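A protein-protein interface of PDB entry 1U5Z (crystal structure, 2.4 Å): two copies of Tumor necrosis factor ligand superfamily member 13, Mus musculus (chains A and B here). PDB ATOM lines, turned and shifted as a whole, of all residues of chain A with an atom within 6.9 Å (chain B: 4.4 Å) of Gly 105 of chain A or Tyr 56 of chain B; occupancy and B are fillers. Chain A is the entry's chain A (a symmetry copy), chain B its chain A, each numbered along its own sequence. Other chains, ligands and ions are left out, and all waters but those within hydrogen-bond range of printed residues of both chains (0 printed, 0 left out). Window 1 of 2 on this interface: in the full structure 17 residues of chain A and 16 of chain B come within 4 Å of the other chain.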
ATOM      1  N   TYR A  53      12.175   6.713  23.655  1.00  0.00           N
ATOM      2  CA  TYR A  53      12.744   7.802  22.834  1.00  0.00           C
ATOM      3  C   TYR A  53      13.586   7.218  21.708  1.00  0.00           C
ATOM      4  O   TYR A  53      14.297   6.237  21.912  1.00  0.00           O
ATOM      5  CB  TYR A  53      13.688   8.711  23.649  1.00  0.00           C
ATOM      6  CG  TYR A  53      13.044   9.560  24.725  1.00  0.00           C
ATOM      7  CD1 TYR A  53      12.836   9.063  26.005  1.00  0.00           C
ATOM      8  CD2 TYR A  53      12.653  10.865  24.458  1.00  0.00           C
ATOM      9  CE1 TYR A  53      12.250   9.850  26.989  1.00  0.00           C
ATOM     10  CE2 TYR A  53      12.051  11.647  25.421  1.00  0.00           C
ATOM     11  CZ  TYR A  53      11.861  11.145  26.687  1.00  0.00           C
ATOM     12  OH  TYR A  53      11.274  11.942  27.646  1.00  0.00           O
ATOM     13  N   LEU A  54      13.477   7.823  20.525  1.00  0.00           N
ATOM     14  CA  LEU A  54      14.483   7.720  19.488  1.00  0.00           C
ATOM     15  C   LEU A  54      15.610   8.674  19.855  1.00  0.00           C
ATOM     16  O   LEU A  54      15.376   9.844  20.123  1.00  0.00           O
ATOM     17  CB  LEU A  54      13.912   8.146  18.142  1.00  0.00           C
ATOM     18  CG  LEU A  54      14.909   8.227  16.975  1.00  0.00           C
ATOM     19  CD1 LEU A  54      15.483   6.858  16.664  1.00  0.00           C
ATOM     20  CD2 LEU A  54      14.215   8.813  15.761  1.00  0.00           C
ATOM     21  N   LEU A  55      16.835   8.173  19.835  1.00  0.00           N
ATOM     22  CA  LEU A  55      17.991   8.960  20.188  1.00  0.00           C
ATOM     23  C   LEU A  55      19.021   8.798  19.075  1.00  0.00           C
ATOM     24  O   LEU A  55      19.357   7.686  18.685  1.00  0.00           O
ATOM     25  CB  LEU A  55      18.503   8.466  21.537  1.00  0.00           C
ATOM     26  CG  LEU A  55      19.777   8.995  22.163  1.00  0.00           C
ATOM     27  CD1 LEU A  55      19.753  10.481  22.166  1.00  0.00           C
ATOM     28  CD2 LEU A  55      19.910   8.423  23.585  1.00  0.00           C
ATOM     29  N   TYR A  56      19.488   9.915  18.528  1.00  0.00           N
ATOM     30  CA  TYR A  56      20.439   9.884  17.429  1.00  0.00           C
ATOM     31  C   TYR A  56      21.611  10.795  17.731  1.00  0.00           C
ATOM     32  O   TYR A  56      21.464  11.798  18.383  1.00  0.00           O
ATOM     33  CB  TYR A  56      19.766  10.277  16.115  1.00  0.00           C
ATOM     34  CG  TYR A  56      19.134  11.643  16.086  1.00  0.00           C
ATOM     35  CD1 TYR A  56      19.868  12.762  15.705  1.00  0.00           C
ATOM     36  CD2 TYR A  56      17.787  11.819  16.423  1.00  0.00           C
ATOM     37  CE1 TYR A  56      19.287  14.023  15.664  1.00  0.00           C
ATOM     38  CE2 TYR A  56      17.193  13.080  16.383  1.00  0.00           C
ATOM     39  CZ  TYR A  56      17.948  14.174  16.004  1.00  0.00           C
ATOM     40  OH  TYR A  56      17.370  15.416  15.957  1.00  0.00           O
ATOM     41  N   SER A  57      22.781  10.423  17.244  1.00  0.00           N
ATOM     42  CA  SER A  57      24.013  11.127  17.547  1.00  0.00           C
ATOM     43  C   SER A  57      24.941  11.086  16.356  1.00  0.00           C
ATOM     44  O   SER A  57      25.277  10.006  15.884  1.00  0.00           O
ATOM     45  CB  SER A  57      24.716  10.441  18.715  1.00  0.00           C
ATOM     46  OG  SER A  57      26.059  10.845  18.774  1.00  0.00           O
ATOM     47  N   PHE A  84      24.178   2.802  22.647  1.00  0.00           N
ATOM     48  CA  PHE A  84      24.825   2.472  21.385  1.00  0.00           C
ATOM     49  C   PHE A  84      26.150   3.205  21.203  1.00  0.00           C
ATOM     50  O   PHE A  84      26.462   4.134  21.925  1.00  0.00           O
ATOM     51  CB  PHE A  84      23.901   2.780  20.205  1.00  0.00           C
ATOM     52  CG  PHE A  84      23.483   4.201  20.122  1.00  0.00           C
ATOM     53  CD1 PHE A  84      22.441   4.667  20.902  1.00  0.00           C
ATOM     54  CD2 PHE A  84      24.122   5.083  19.261  1.00  0.00           C
ATOM     55  CE1 PHE A  84      22.037   5.998  20.831  1.00  0.00           C
ATOM     56  CE2 PHE A  84      23.727   6.411  19.184  1.00  0.00           C
ATOM     57  CZ  PHE A  84      22.683   6.872  19.969  1.00  0.00           C
ATOM     58  N   SER A 103      25.072   7.177  14.491  1.00  0.00           N
ATOM     59  CA  SER A 103      24.290   6.036  14.958  1.00  0.00           C
ATOM     60  C   SER A 103      23.034   6.524  15.678  1.00  0.00           C
ATOM     61  O   SER A 103      22.926   7.703  16.020  1.00  0.00           O
ATOM     62  CB  SER A 103      25.126   5.137  15.866  1.00  0.00           C
ATOM     63  OG  SER A 103      24.359   4.039  16.336  1.00  0.00           O
ATOM     64  N   ALA A 104      22.085   5.608  15.879  1.00  0.00           N
ATOM     65  CA  ALA A 104      20.818   5.919  16.529  1.00  0.00           C
ATOM     66  C   ALA A 104      20.067   4.663  16.945  1.00  0.00           C
ATOM     67  O   ALA A 104      20.242   3.599  16.361  1.00  0.00           O
ATOM     68  CB  ALA A 104      19.937   6.751  15.596  1.00  0.00           C
ATOM     69  N   GLY A 105      19.215   4.790  17.955  1.00  0.00           N
ATOM     70  CA  GLY A 105      18.331   3.709  18.338  1.00  0.00           C
ATOM     71  C   GLY A 105      17.187   4.183  19.210  1.00  0.00           C
ATOM     72  O   GLY A 105      17.093   5.360  19.555  1.00  0.00           O
ATOM     73  N   VAL A 106      16.323   3.244  19.575  1.00  0.00           N
ATOM     74  CA  VAL A 106      15.151   3.525  20.380  1.00  0.00           C
ATOM     75  C   VAL A 106      15.333   2.854  21.744  1.00  0.00           C
ATOM     76  O   VAL A 106      15.700   1.680  21.833  1.00  0.00           O
ATOM     77  CB  VAL A 106      13.874   3.040  19.670  1.00  0.00           C
ATOM     78  CG1 VAL A 106      12.653   3.369  20.481  1.00  0.00           C
ATOM     79  CG2 VAL A 106      13.755   3.681  18.282  1.00  0.00           C
ATOM     80  N   PHE A 107      15.086   3.616  22.801  1.00  0.00           N
ATOM     81  CA  PHE A 107      15.438   3.216  24.156  1.00  0.00           C
ATOM     82  C   PHE A 107      14.467   3.737  25.204  1.00  0.00           C
ATOM     83  O   PHE A 107      13.970   4.869  25.117  1.00  0.00           O
ATOM     84  CB  PHE A 107      16.839   3.728  24.496  1.00  0.00           C
ATOM     85  CG  PHE A 107      17.910   3.154  23.626  1.00  0.00           C
ATOM     86  CD1 PHE A 107      18.394   1.887  23.865  1.00  0.00           C
ATOM     87  CD2 PHE A 107      18.425   3.880  22.561  1.00  0.00           C
ATOM     88  CE1 PHE A 107      19.375   1.344  23.069  1.00  0.00           C
ATOM     89  CE2 PHE A 107      19.401   3.339  21.756  1.00  0.00           C
ATOM     90  CZ  PHE A 107      19.881   2.063  22.016  1.00  0.00           C
ATOM     91  N   LEU B   8      10.246  -2.107  18.567  1.00  0.00           N
ATOM     92  CA  LEU B   8      11.011  -3.317  18.825  1.00  0.00           C
ATOM     93  C   LEU B   8      12.493  -3.038  18.588  1.00  0.00           C
ATOM     94  O   LEU B   8      12.864  -2.579  17.533  1.00  0.00           O
ATOM     95  CB  LEU B   8      10.535  -4.451  17.912  1.00  0.00           C
ATOM     96  CG  LEU B   8      11.102  -5.857  18.135  1.00  0.00           C
ATOM     97  CD1 LEU B   8      10.683  -6.407  19.486  1.00  0.00           C
ATOM     98  CD2 LEU B   8      10.641  -6.790  17.018  1.00  0.00           C
ATOM     99  N   HIS B   9      13.324  -3.303  19.589  1.00  0.00           N
ATOM    100  CA  HIS B   9      14.767  -3.148  19.489  1.00  0.00           C
ATOM    101  C   HIS B   9      15.361  -4.505  19.792  1.00  0.00           C
ATOM    102  O   HIS B   9      15.083  -5.087  20.832  1.00  0.00           O
ATOM    103  CB  HIS B   9      15.254  -2.104  20.496  1.00  0.00           C
ATOM    104  CG  HIS B   9      16.710  -1.756  20.378  1.00  0.00           C
ATOM    105  ND1 HIS B   9      17.209  -0.968  19.363  1.00  0.00           N
ATOM    106  CD2 HIS B   9      17.763  -2.043  21.182  1.00  0.00           C
ATOM    107  CE1 HIS B   9      18.511  -0.809  19.532  1.00  0.00           C
ATOM    108  NE2 HIS B   9      18.868  -1.430  20.642  1.00  0.00           N
ATOM    109  N   LEU B  54       9.559   2.665  10.516  1.00  0.00           N
ATOM    110  CA  LEU B  54      10.960   3.032  10.514  1.00  0.00           C
ATOM    111  C   LEU B  54      11.753   1.789  10.889  1.00  0.00           C
ATOM    112  O   LEU B  54      11.471   1.147  11.890  1.00  0.00           O
ATOM    113  CB  LEU B  54      11.234   4.110  11.553  1.00  0.00           C
ATOM    114  CG  LEU B  54      12.709   4.493  11.763  1.00  0.00           C
ATOM    115  CD1 LEU B  54      13.289   5.105  10.503  1.00  0.00           C
ATOM    116  CD2 LEU B  54      12.816   5.453  12.932  1.00  0.00           C
ATOM    117  N   LEU B  55      12.765   1.475  10.096  1.00  0.00           N
ATOM    118  CA  LEU B  55      13.582   0.308  10.320  1.00  0.00           C
ATOM    119  C   LEU B  55      15.041   0.748  10.287  1.00  0.00           C
ATOM    120  O   LEU B  55      15.478   1.409   9.352  1.00  0.00           O
ATOM    121  CB  LEU B  55      13.253  -0.714   9.237  1.00  0.00           C
ATOM    122  CG  LEU B  55      14.006  -2.020   9.099  1.00  0.00           C
ATOM    123  CD1 LEU B  55      14.060  -2.708  10.415  1.00  0.00           C
ATOM    124  CD2 LEU B  55      13.317  -2.885   8.030  1.00  0.00           C
ATOM    125  N   TYR B  56      15.787   0.422  11.337  1.00  0.00           N
ATOM    126  CA  TYR B  56      17.179   0.827  11.437  1.00  0.00           C
ATOM    127  C   TYR B  56      18.043  -0.367  11.785  1.00  0.00           C
ATOM    128  O   TYR B  56      17.618  -1.261  12.472  1.00  0.00           O
ATOM    129  CB  TYR B  56      17.350   1.943  12.465  1.00  0.00           C
ATOM    130  CG  TYR B  56      16.905   1.616  13.866  1.00  0.00           C
ATOM    131  CD1 TYR B  56      17.784   1.041  14.779  1.00  0.00           C
ATOM    132  CD2 TYR B  56      15.602   1.900  14.291  1.00  0.00           C
ATOM    133  CE1 TYR B  56      17.384   0.748  16.076  1.00  0.00           C
ATOM    134  CE2 TYR B  56      15.191   1.612  15.592  1.00  0.00           C
ATOM    135  CZ  TYR B  56      16.085   1.038  16.477  1.00  0.00           C
ATOM    136  OH  TYR B  56      15.690   0.757  17.758  1.00  0.00           O
ATOM    137  N   SER B  57      19.269  -0.364  11.294  1.00  0.00           N
ATOM    138  CA  SER B  57      20.173  -1.490  11.442  1.00  0.00           C
ATOM    139  C   SER B  57      21.596  -1.000  11.574  1.00  0.00           C
ATOM    140  O   SER B  57      22.079  -0.293  10.696  1.00  0.00           O
ATOM    141  CB  SER B  57      20.092  -2.372  10.199  1.00  0.00           C
ATOM    142  OG  SER B  57      21.206  -3.225  10.141  1.00  0.00           O
ATOM    143  N   TYR B 102      25.911   1.995   9.734  1.00  0.00           N
ATOM    144  CA  TYR B 102      24.540   2.303  10.119  1.00  0.00           C
ATOM    145  C   TYR B 102      23.728   2.708   8.893  1.00  0.00           C
ATOM    146  O   TYR B 102      24.182   3.502   8.076  1.00  0.00           O
ATOM    147  CB  TYR B 102      24.523   3.442  11.157  1.00  0.00           C
ATOM    148  CG  TYR B 102      23.140   3.739  11.705  1.00  0.00           C
ATOM    149  CD1 TYR B 102      22.251   4.552  11.004  1.00  0.00           C
ATOM    150  CD2 TYR B 102      22.715   3.191  12.897  1.00  0.00           C
ATOM    151  CE1 TYR B 102      20.985   4.819  11.484  1.00  0.00           C
ATOM    152  CE2 TYR B 102      21.434   3.448  13.390  1.00  0.00           C
ATOM    153  CZ  TYR B 102      20.581   4.267  12.677  1.00  0.00           C
ATOM    154  OH  TYR B 102      19.322   4.533  13.140  1.00  0.00           O
ATOM    155  N   SER B 103      22.520   2.178   8.776  1.00  0.00           N
ATOM    156  CA  SER B 103      21.553   2.720   7.827  1.00  0.00           C
ATOM    157  C   SER B 103      20.134   2.527   8.359  1.00  0.00           C
ATOM    158  O   SER B 103      19.918   1.766   9.305  1.00  0.00           O
ATOM    159  CB  SER B 103      21.714   2.072   6.453  1.00  0.00           C
ATOM    160  OG  SER B 103      20.760   2.585   5.536  1.00  0.00           O
ATOM    161  N   ALA B 104      19.182   3.242   7.755  1.00  0.00           N
ATOM    162  CA  ALA B 104      17.784   3.189   8.161  1.00  0.00           C
ATOM    163  C   ALA B 104      16.865   3.810   7.120  1.00  0.00           C
ATOM    164  O   ALA B 104      17.275   4.668   6.346  1.00  0.00           O
ATOM    165  CB  ALA B 104      17.595   3.909   9.497  1.00  0.00           C
ATOM    166  N   PHE B 134      22.742  -4.042  16.223  1.00  0.00           N
ATOM    167  CA  PHE B 134      21.347  -3.991  16.634  1.00  0.00           C
ATOM    168  C   PHE B 134      20.403  -3.669  15.481  1.00  0.00           C
ATOM    169  O   PHE B 134      20.770  -2.993  14.527  1.00  0.00           O
ATOM    170  CB  PHE B 134      21.152  -2.965  17.768  1.00  0.00           C
ATOM    171  CG  PHE B 134      21.665  -1.569  17.448  1.00  0.00           C
ATOM    172  CD1 PHE B 134      20.940  -0.717  16.630  1.00  0.00           C
ATOM    173  CD2 PHE B 134      22.854  -1.101  18.006  1.00  0.00           C
ATOM    174  CE1 PHE B 134      21.403   0.586  16.360  1.00  0.00           C
ATOM    175  CE2 PHE B 134      23.318   0.203  17.743  1.00  0.00           C
ATOM    176  CZ  PHE B 134      22.599   1.038  16.921  1.00  0.00           C
ATOM    177  N   LEU B 135      19.179  -4.167  15.590  1.00  0.00           N
ATOM    178  CA  LEU B 135      18.141  -3.966  14.586  1.00  0.00           C
ATOM    179  C   LEU B 135      16.916  -3.442  15.308  1.00  0.00           C
ATOM    180  O   LEU B 135      16.641  -3.872  16.428  1.00  0.00           O
ATOM    181  CB  LEU B 135      17.824  -5.299  13.918  1.00  0.00           C
ATOM    182  CG  LEU B 135      16.684  -5.388  12.902  1.00  0.00           C
ATOM    183  CD1 LEU B 135      17.001  -4.537  11.679  1.00  0.00           C
ATOM    184  CD2 LEU B 135      16.447  -6.875  12.522  1.00  0.00           C
ATOM    185  N   GLY B 136      16.166  -2.540  14.682  1.00  0.00           N
ATOM    186  CA  GLY B 136      15.015  -1.935  15.352  1.00  0.00           C
ATOM    187  C   GLY B 136      13.870  -1.436  14.479  1.00  0.00           C
ATOM    188  O   GLY B 136      14.051  -1.209  13.278  1.00  0.00           O
ATOM    189  N   PHE B 137      12.699  -1.258  15.110  1.00  0.00           N
ATOM    190  CA  PHE B 137      11.447  -0.943  14.421  1.00  0.00           C
ATOM    191  C   PHE B 137      10.600   0.070  15.220  1.00  0.00           C
ATOM    192  O   PHE B 137      10.483  -0.021  16.442  1.00  0.00           O
ATOM    193  CB  PHE B 137      10.578  -2.209  14.230  1.00  0.00           C
ATOM    194  CG  PHE B 137      11.269  -3.339  13.545  1.00  0.00           C
ATOM    195  CD1 PHE B 137      12.088  -4.201  14.258  1.00  0.00           C
ATOM    196  CD2 PHE B 137      11.068  -3.571  12.188  1.00  0.00           C
ATOM    197  CE1 PHE B 137      12.723  -5.269  13.616  1.00  0.00           C
ATOM    198  CE2 PHE B 137      11.693  -4.627  11.544  1.00  0.00           C
ATOM    199  CZ  PHE B 137      12.523  -5.475  12.254  1.00  0.00           C
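OH of Tyr 102 of chain B lies close to O of Ala 104 of chain A, 3.5 Å away. The side-chain hydroxyl (OH) of Tyr 56 of chain B lies within hydrogen-bond range of the backbone NH (N) of Val 106 of chain A, 3.1 Å away.
Hydrophobic or aromatic side chains of chain B that line the printed part of chain A: His 9, Tyr 56, Tyr 102 and Phe 134. Printed residues of chain A that touch a printed residue of chain B: Phe 84, Ser 103, Ala 104, Gly 105, Val 106 and Phe 107. Hydrophobic or aromatic side chains of chain A within 4 Å of the printed part of chain B: Phe 84, Ala 104, Val 106 and Phe 107. Among the printed residues, no Asp or Glu carboxylate lies within 4 Å of a Lys or Arg side-chain nitrogen of the other chain.
Ala 104 of chain A touches Tyr 56 of chain B, but with the chains exchanged Tyr 56 of chain A does not touch Ala 104 of chain B (9.4 Å). 6 positions are printed for both chains. Of the 10 pairs that touch across the chains among the printed residues, none has its exchanged pair printed and touching as well.
A ring nitrogen (ND1) of His 9 of chain B lies within hydrogen-bond range of the side-chain hydroxyl (OH) of Tyr 56 of chain B, 2.8 Å away. The backbone NH of Phe 107 of chain A is in hydrogen-bond range of the backbone carbonyl oxygen of Tyr 53 of chain A (2.9 Å). The backbone carbonyl oxygen (O) of Gly 105 of chain A is in hydrogen-bond range of the backbone NH (N) of Leu 55 of chain A (2.8 Å). The backbone carbonyl oxygen (O) of Tyr 56 of chain B sits at hydrogen-bond distance from the backbone NH (N) of Gly 136 of chain B, 2.9 Å away. The backbone carbonyl oxygen (O) of Ser 103 of chain A sits at hydrogen-bond distance from the backbone NH (N) of Ser 57 of chain A (3.0 Å).
Among the printed residues, merely in contact across the chains: Ala 104 of chain A with Phe 134 of chain B (3.2 Å), Ser 103 of chain A with Phe 134 of chain B (3.5 Å), Phe 84 of chain A with Phe 134 of chain B (3.6 Å), Phe 107 of chain A with His 9 of chain B (3.7 Å), Gly 105 of chain A with Tyr 56 of chain B (3.8 Å), Ser 103 of chain A with Tyr 102 of chain B (3.8 Å), Val 106 of chain A with His 9 of chain B (3.9 Å) and Ala 104 of chain A with Tyr 56 of chain B (3.9 Å).
Tyr 53 of chain A touches none of the printed residues of chain B. Printed residues of chain B within 4 Å of Ala 104 of chain A: Tyr 56, Tyr 102 and Phe 134. Gly 105 of chain A touches just one residue of chain B: Tyr 56. Tyr 56 of chain B touches three residues of chain A. Printed residues of chain A within 4 Å of Tyr 102 of chain B: Ser 103 (3.8 Å) and Ala 104 (3.2 Å). The nearest printed residue of chain B that does not touch Gly 105 of chain A is His 9 of chain B (4.7 Å). The nearest residue of chain A that does not touch Tyr 56 of chain B is Leu 54 of chain A (5.4 Å).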
